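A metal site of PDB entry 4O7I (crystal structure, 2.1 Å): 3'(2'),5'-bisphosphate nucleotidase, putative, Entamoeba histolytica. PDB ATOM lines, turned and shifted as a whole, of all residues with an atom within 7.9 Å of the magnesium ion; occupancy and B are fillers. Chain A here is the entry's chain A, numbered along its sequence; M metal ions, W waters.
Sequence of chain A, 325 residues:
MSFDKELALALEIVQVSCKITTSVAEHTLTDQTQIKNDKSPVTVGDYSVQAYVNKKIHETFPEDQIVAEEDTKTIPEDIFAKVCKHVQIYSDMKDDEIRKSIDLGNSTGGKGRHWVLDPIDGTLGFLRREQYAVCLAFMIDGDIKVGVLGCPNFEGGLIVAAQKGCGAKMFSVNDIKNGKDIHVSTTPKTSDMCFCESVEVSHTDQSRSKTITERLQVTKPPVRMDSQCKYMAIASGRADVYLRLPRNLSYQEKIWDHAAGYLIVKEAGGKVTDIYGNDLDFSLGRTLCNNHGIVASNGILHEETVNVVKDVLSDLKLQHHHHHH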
ATOM      1  N   LYS A  36      -0.260   0.240  20.298  1.00  0.00           N
ATOM      2  CA  LYS A  36       1.052   0.012  20.893  1.00  0.00           C
ATOM      3  C   LYS A  36       1.406  -1.478  20.835  1.00  0.00           C
ATOM      4  O   LYS A  36       0.577  -2.305  20.421  1.00  0.00           O
ATOM      5  CB  LYS A  36       1.085   0.514  22.356  1.00  0.00           C
ATOM      6  CG  LYS A  36       0.646   1.966  22.528  1.00  0.00           C
ATOM      7  CD  LYS A  36       1.155   2.625  23.822  1.00  0.00           C
ATOM      8  CE  LYS A  36       0.170   2.538  24.967  1.00  0.00           C
ATOM      9  NZ  LYS A  36       0.704   3.173  26.201  1.00  0.00           N
ATOM     10  N   PRO A  41      -4.508   0.743  22.875  1.00  0.00           N
ATOM     11  CA  PRO A  41      -4.556   1.905  21.993  1.00  0.00           C
ATOM     12  C   PRO A  41      -4.006   3.154  22.618  1.00  0.00           C
ATOM     13  O   PRO A  41      -4.068   3.306  23.839  1.00  0.00           O
ATOM     14  CB  PRO A  41      -6.048   2.106  21.738  1.00  0.00           C
ATOM     15  CG  PRO A  41      -6.696   1.591  22.973  1.00  0.00           C
ATOM     16  CD  PRO A  41      -5.854   0.413  23.407  1.00  0.00           C
ATOM     17  N   VAL A  42      -3.465   4.018  21.769  1.00  0.00           N
ATOM     18  CA  VAL A  42      -3.151   5.395  22.150  1.00  0.00           C
ATOM     19  C   VAL A  42      -3.606   6.304  20.986  1.00  0.00           C
ATOM     20  O   VAL A  42      -3.451   5.945  19.816  1.00  0.00           O
ATOM     21  CB  VAL A  42      -1.646   5.569  22.483  1.00  0.00           C
ATOM     22  CG1 VAL A  42      -0.760   5.323  21.272  1.00  0.00           C
ATOM     23  CG2 VAL A  42      -1.370   6.944  23.084  1.00  0.00           C
ATOM     24  N   ASP A  46      -4.402  11.384  23.722  1.00  0.00           N
ATOM     25  CA  ASP A  46      -3.512  10.945  24.803  1.00  0.00           C
ATOM     26  C   ASP A  46      -2.204  11.754  24.698  1.00  0.00           C
ATOM     27  O   ASP A  46      -1.730  12.336  25.682  1.00  0.00           O
ATOM     28  CB  ASP A  46      -3.213   9.435  24.718  1.00  0.00           C
ATOM     29  CG  ASP A  46      -4.472   8.550  24.732  1.00  0.00           C
ATOM     30  OD1 ASP A  46      -5.285   8.635  23.784  1.00  0.00           O
ATOM     31  OD2 ASP A  46      -4.617   7.720  25.659  1.00  0.00           O
ATOM     32  N   GLN A  50      -0.785  15.008  27.053  1.00  0.00           N
ATOM     33  CA  GLN A  50       0.484  14.852  27.771  1.00  0.00           C
ATOM     34  C   GLN A  50       1.497  15.950  27.433  1.00  0.00           C
ATOM     35  O   GLN A  50       2.162  16.465  28.319  1.00  0.00           O
ATOM     36  CB  GLN A  50       1.075  13.458  27.531  1.00  0.00           C
ATOM     37  CG  GLN A  50       2.377  13.194  28.300  1.00  0.00           C
ATOM     38  CD  GLN A  50       2.681  11.722  28.479  1.00  0.00           C
ATOM     39  OE1 GLN A  50       1.791  10.922  28.741  1.00  0.00           O
ATOM     40  NE2 GLN A  50       3.954  11.352  28.391  1.00  0.00           N
ATOM     41  N   GLU A  69       2.115   8.303  31.339  1.00  0.00           N
ATOM     42  CA  GLU A  69       2.008   7.003  30.651  1.00  0.00           C
ATOM     43  C   GLU A  69       2.748   6.923  29.295  1.00  0.00           C
ATOM     44  O   GLU A  69       3.437   5.940  29.010  1.00  0.00           O
ATOM     45  CB  GLU A  69       0.539   6.642  30.447  1.00  0.00           C
ATOM     46  CG  GLU A  69       0.334   5.293  29.770  1.00  0.00           C
ATOM     47  CD  GLU A  69      -1.114   4.915  29.600  1.00  0.00           C
ATOM     48  OE1 GLU A  69      -2.013   5.791  29.712  1.00  0.00           O
ATOM     49  OE2 GLU A  69      -1.363   3.721  29.362  1.00  0.00           O
ATOM     50  N   GLU A  70       2.584   7.945  28.468  1.00  0.00           N
ATOM     51  CA  GLU A  70       3.002   7.828  27.076  1.00  0.00           C
ATOM     52  C   GLU A  70       4.435   8.312  26.873  1.00  0.00           C
ATOM     53  O   GLU A  70       5.015   8.969  27.738  1.00  0.00           O
ATOM     54  CB  GLU A  70       2.030   8.589  26.171  1.00  0.00           C
ATOM     55  CG  GLU A  70       0.553   8.306  26.434  1.00  0.00           C
ATOM     56  CD  GLU A  70       0.149   6.851  26.255  1.00  0.00           C
ATOM     57  OE1 GLU A  70       0.944   6.023  25.752  1.00  0.00           O
ATOM     58  OE2 GLU A  70      -1.004   6.540  26.629  1.00  0.00           O
ATOM     59  N   LEU A 117       0.431  11.510  35.784  1.00  0.00           N
ATOM     60  CA  LEU A 117      -0.464  11.912  34.705  1.00  0.00           C
ATOM     61  C   LEU A 117      -0.851  10.718  33.883  1.00  0.00           C
ATOM     62  O   LEU A 117       0.008   9.984  33.423  1.00  0.00           O
ATOM     63  CB  LEU A 117       0.191  12.924  33.755  1.00  0.00           C
ATOM     64  CG  LEU A 117      -0.606  13.244  32.461  1.00  0.00           C
ATOM     65  CD1 LEU A 117      -1.886  14.000  32.788  1.00  0.00           C
ATOM     66  CD2 LEU A 117       0.192  14.032  31.442  1.00  0.00           C
ATOM     67  N   ASP A 118      -2.157  10.519  33.725  1.00  0.00           N
ATOM     68  CA  ASP A 118      -2.673   9.668  32.676  1.00  0.00           C
ATOM     69  C   ASP A 118      -3.446  10.590  31.737  1.00  0.00           C
ATOM     70  O   ASP A 118      -4.551  11.015  32.075  1.00  0.00           O
ATOM     71  CB  ASP A 118      -3.606   8.613  33.253  1.00  0.00           C
ATOM     72  CG  ASP A 118      -3.949   7.539  32.256  1.00  0.00           C
ATOM     73  OD1 ASP A 118      -3.687   7.721  31.029  1.00  0.00           O
ATOM     74  OD2 ASP A 118      -4.453   6.486  32.701  1.00  0.00           O
ATOM     75  N   PRO A 119      -2.860  10.905  30.568  1.00  0.00           N
ATOM     76  CA  PRO A 119      -3.464  11.957  29.736  1.00  0.00           C
ATOM     77  C   PRO A 119      -4.863  11.583  29.257  1.00  0.00           C
ATOM     78  O   PRO A 119      -5.744  12.441  29.190  1.00  0.00           O
ATOM     79  CB  PRO A 119      -2.466  12.121  28.596  1.00  0.00           C
ATOM     80  CG  PRO A 119      -1.732  10.818  28.514  1.00  0.00           C
ATOM     81  CD  PRO A 119      -1.651  10.319  29.921  1.00  0.00           C
ATOM     82  N   ILE A 120      -5.061  10.300  28.932  1.00  0.00           N
ATOM     83  CA  ILE A 120      -6.405   9.733  28.869  1.00  0.00           C
ATOM     84  C   ILE A 120      -6.407   8.372  29.579  1.00  0.00           C
ATOM     85  O   ILE A 120      -5.782   7.389  29.146  1.00  0.00           O
ATOM     86  CB  ILE A 120      -6.913   9.573  27.412  1.00  0.00           C
ATOM     87  CG1 ILE A 120      -7.052  10.944  26.723  1.00  0.00           C
ATOM     88  CG2 ILE A 120      -8.234   8.808  27.376  1.00  0.00           C
ATOM     89  CD1 ILE A 120      -7.482  10.872  25.266  1.00  0.00           C
ATOM     90  N   ASP A 121      -7.125   8.356  30.695  1.00  0.00           N
ATOM     91  CA  ASP A 121      -7.397   7.163  31.443  1.00  0.00           C
ATOM     92  C   ASP A 121      -8.651   6.556  30.821  1.00  0.00           C
ATOM     93  O   ASP A 121      -9.675   7.230  30.701  1.00  0.00           O
ATOM     94  CB  ASP A 121      -7.629   7.545  32.897  1.00  0.00           C
ATOM     95  CG  ASP A 121      -7.613   6.367  33.833  1.00  0.00           C
ATOM     96  OD1 ASP A 121      -8.574   5.560  33.832  1.00  0.00           O
ATOM     97  OD2 ASP A 121      -6.634   6.251  34.590  1.00  0.00           O
ATOM     98  N   GLY A 122      -8.581   5.307  30.394  1.00  0.00           N
ATOM     99  CA  GLY A 122      -9.742   4.696  29.735  1.00  0.00           C
ATOM    100  C   GLY A 122      -9.839   5.110  28.273  1.00  0.00           C
ATOM    101  O   GLY A 122     -10.902   5.545  27.801  1.00  0.00           O
ATOM    102  N   THR A 123      -8.731   4.948  27.561  1.00  0.00           N
ATOM    103  CA  THR A 123      -8.662   5.250  26.126  1.00  0.00           C
ATOM    104  C   THR A 123      -9.658   4.413  25.320  1.00  0.00           C
ATOM    105  O   THR A 123     -10.167   4.899  24.315  1.00  0.00           O
ATOM    106  CB  THR A 123      -7.220   5.060  25.544  1.00  0.00           C
ATOM    107  OG1 THR A 123      -6.267   5.799  26.337  1.00  0.00           O
ATOM    108  CG2 THR A 123      -7.119   5.560  24.072  1.00  0.00           C
ATOM    109  N   LEU A 124      -9.921   3.175  25.728  1.00  0.00           N
ATOM    110  CA  LEU A 124     -11.013   2.387  25.104  1.00  0.00           C
ATOM    111  C   LEU A 124     -12.368   3.075  25.328  1.00  0.00           C
ATOM    112  O   LEU A 124     -13.207   3.091  24.428  1.00  0.00           O
ATOM    113  CB  LEU A 124     -11.027   0.959  25.625  1.00  0.00           C
ATOM    114  CG  LEU A 124      -9.895   0.068  25.071  1.00  0.00           C
ATOM    115  CD1 LEU A 124      -9.810  -1.231  25.863  1.00  0.00           C
ATOM    116  CD2 LEU A 124     -10.056  -0.205  23.567  1.00  0.00           C
ATOM    117  N   ALA A 133     -11.270   9.751  31.363  1.00  0.00           N
ATOM    118  CA  ALA A 133     -10.842  10.766  32.342  1.00  0.00           C
ATOM    119  C   ALA A 133      -9.464  11.277  32.002  1.00  0.00           C
ATOM    120  O   ALA A 133      -8.611  10.511  31.585  1.00  0.00           O
ATOM    121  CB  ALA A 133     -10.826  10.177  33.737  1.00  0.00           C
ATOM    122  N   CYS A 135      -6.505  12.349  34.128  1.00  0.00           N
ATOM    123  CA  CYS A 135      -6.124  12.176  35.524  1.00  0.00           C
ATOM    124  C   CYS A 135      -4.776  12.791  35.838  1.00  0.00           C
ATOM    125  O   CYS A 135      -3.782  12.462  35.189  1.00  0.00           O
ATOM    126  CB  CYS A 135      -6.152  10.682  35.887  1.00  0.00           C
ATOM    127  SG  CYS A 135      -7.689   9.879  35.306  1.00  0.00           S
ATOM    128  N   TRP A 256      -0.786   5.825  37.739  1.00  0.00           N
ATOM    129  CA  TRP A 256      -1.617   6.797  36.996  1.00  0.00           C
ATOM    130  C   TRP A 256      -3.023   6.267  36.686  1.00  0.00           C
ATOM    131  O   TRP A 256      -3.844   6.983  36.121  1.00  0.00           O
ATOM    132  CB  TRP A 256      -0.918   7.258  35.717  1.00  0.00           C
ATOM    133  CG  TRP A 256      -0.566   6.130  34.772  1.00  0.00           C
ATOM    134  CD1 TRP A 256      -1.432   5.346  34.052  1.00  0.00           C
ATOM    135  CD2 TRP A 256       0.745   5.655  34.455  1.00  0.00           C
ATOM    136  NE1 TRP A 256      -0.732   4.425  33.298  1.00  0.00           N
ATOM    137  CE2 TRP A 256       0.605   4.579  33.540  1.00  0.00           C
ATOM    138  CE3 TRP A 256       2.029   6.027  34.860  1.00  0.00           C
ATOM    139  CZ2 TRP A 256       1.690   3.884  33.026  1.00  0.00           C
ATOM    140  CZ3 TRP A 256       3.101   5.347  34.354  1.00  0.00           C
ATOM    141  CH2 TRP A 256       2.933   4.270  33.444  1.00  0.00           C
ATOM    142  N   ASP A 257      -3.325   5.042  37.076  1.00  0.00           N
ATOM    143  CA  ASP A 257      -4.726   4.567  37.035  1.00  0.00           C
ATOM    144  C   ASP A 257      -5.429   4.674  38.397  1.00  0.00           C
ATOM    145  O   ASP A 257      -6.584   4.281  38.488  1.00  0.00           O
ATOM    146  CB  ASP A 257      -4.777   3.106  36.507  1.00  0.00           C
ATOM    147  CG  ASP A 257      -4.369   2.998  35.028  1.00  0.00           C
ATOM    148  OD1 ASP A 257      -4.448   4.024  34.313  1.00  0.00           O
ATOM    149  OD2 ASP A 257      -3.979   1.884  34.594  1.00  0.00           O
HETATM  150 MG    MG M   1      -3.913   6.324  29.391  1.00  0.00          MG
HETATM  151  O   HOH W   1      -3.137   7.636  28.012  1.00  0.00           O
HETATM  152  O   HOH W   2      -4.356   5.070  27.841  1.00  0.00           O
HETATM  153  O   HOH W   3      -4.767   4.930  30.575  1.00  0.00           O
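Water W1 lies within hydrogen-bond range of OE2 of Glu 70 (2.8 Å), OD2 of Asp 46 (2.8 Å) and N of Ile 120 (3.4 Å). Water W2 bridges OG1 of Thr 123 (2.5 Å) and OD2 of Asp 46 (3.4 Å).
The side-chain carboxylate (OE2) of Glu 69 lies within salt-bridge range of the side-chain amino group (NZ) of Lys 36. The side-chain hydroxyl of Thr 123 lies close to the backbone carbonyl oxygen of Ile 120 (3.3 Å). The side-chain hydroxyl of Thr 123 sits at hydrogen-bond distance from the side-chain carboxylate of Asp 46 (2.6 Å). The backbone NH (N) of Asp 118 is in hydrogen-bond range of the backbone carbonyl oxygen (O) of Cys 135 (2.9 Å). The backbone carbonyl oxygen of Leu 117 sits at hydrogen-bond distance from the backbone NH of Glu 69, at 3.4 Å.
The magnesium ion is bound by the side-chain carboxylate (OE1) of Glu 69, water W3, water W2, water W1, the side-chain carboxylate (OD1) of Asp 118 and the backbone carbonyl oxygen (O) of Ile 120. The magnesium ion has six donor atoms within binding distance.
Merely in contact with the magnesium ion: Thr 123 (3.9 Å). Within 4 Å of the magnesium ion: Glu 69, Asp 118, Ile 120 and Thr 123. The nearest printed residue that does not touch the magnesium ion is Glu 70 (4.02 Å).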
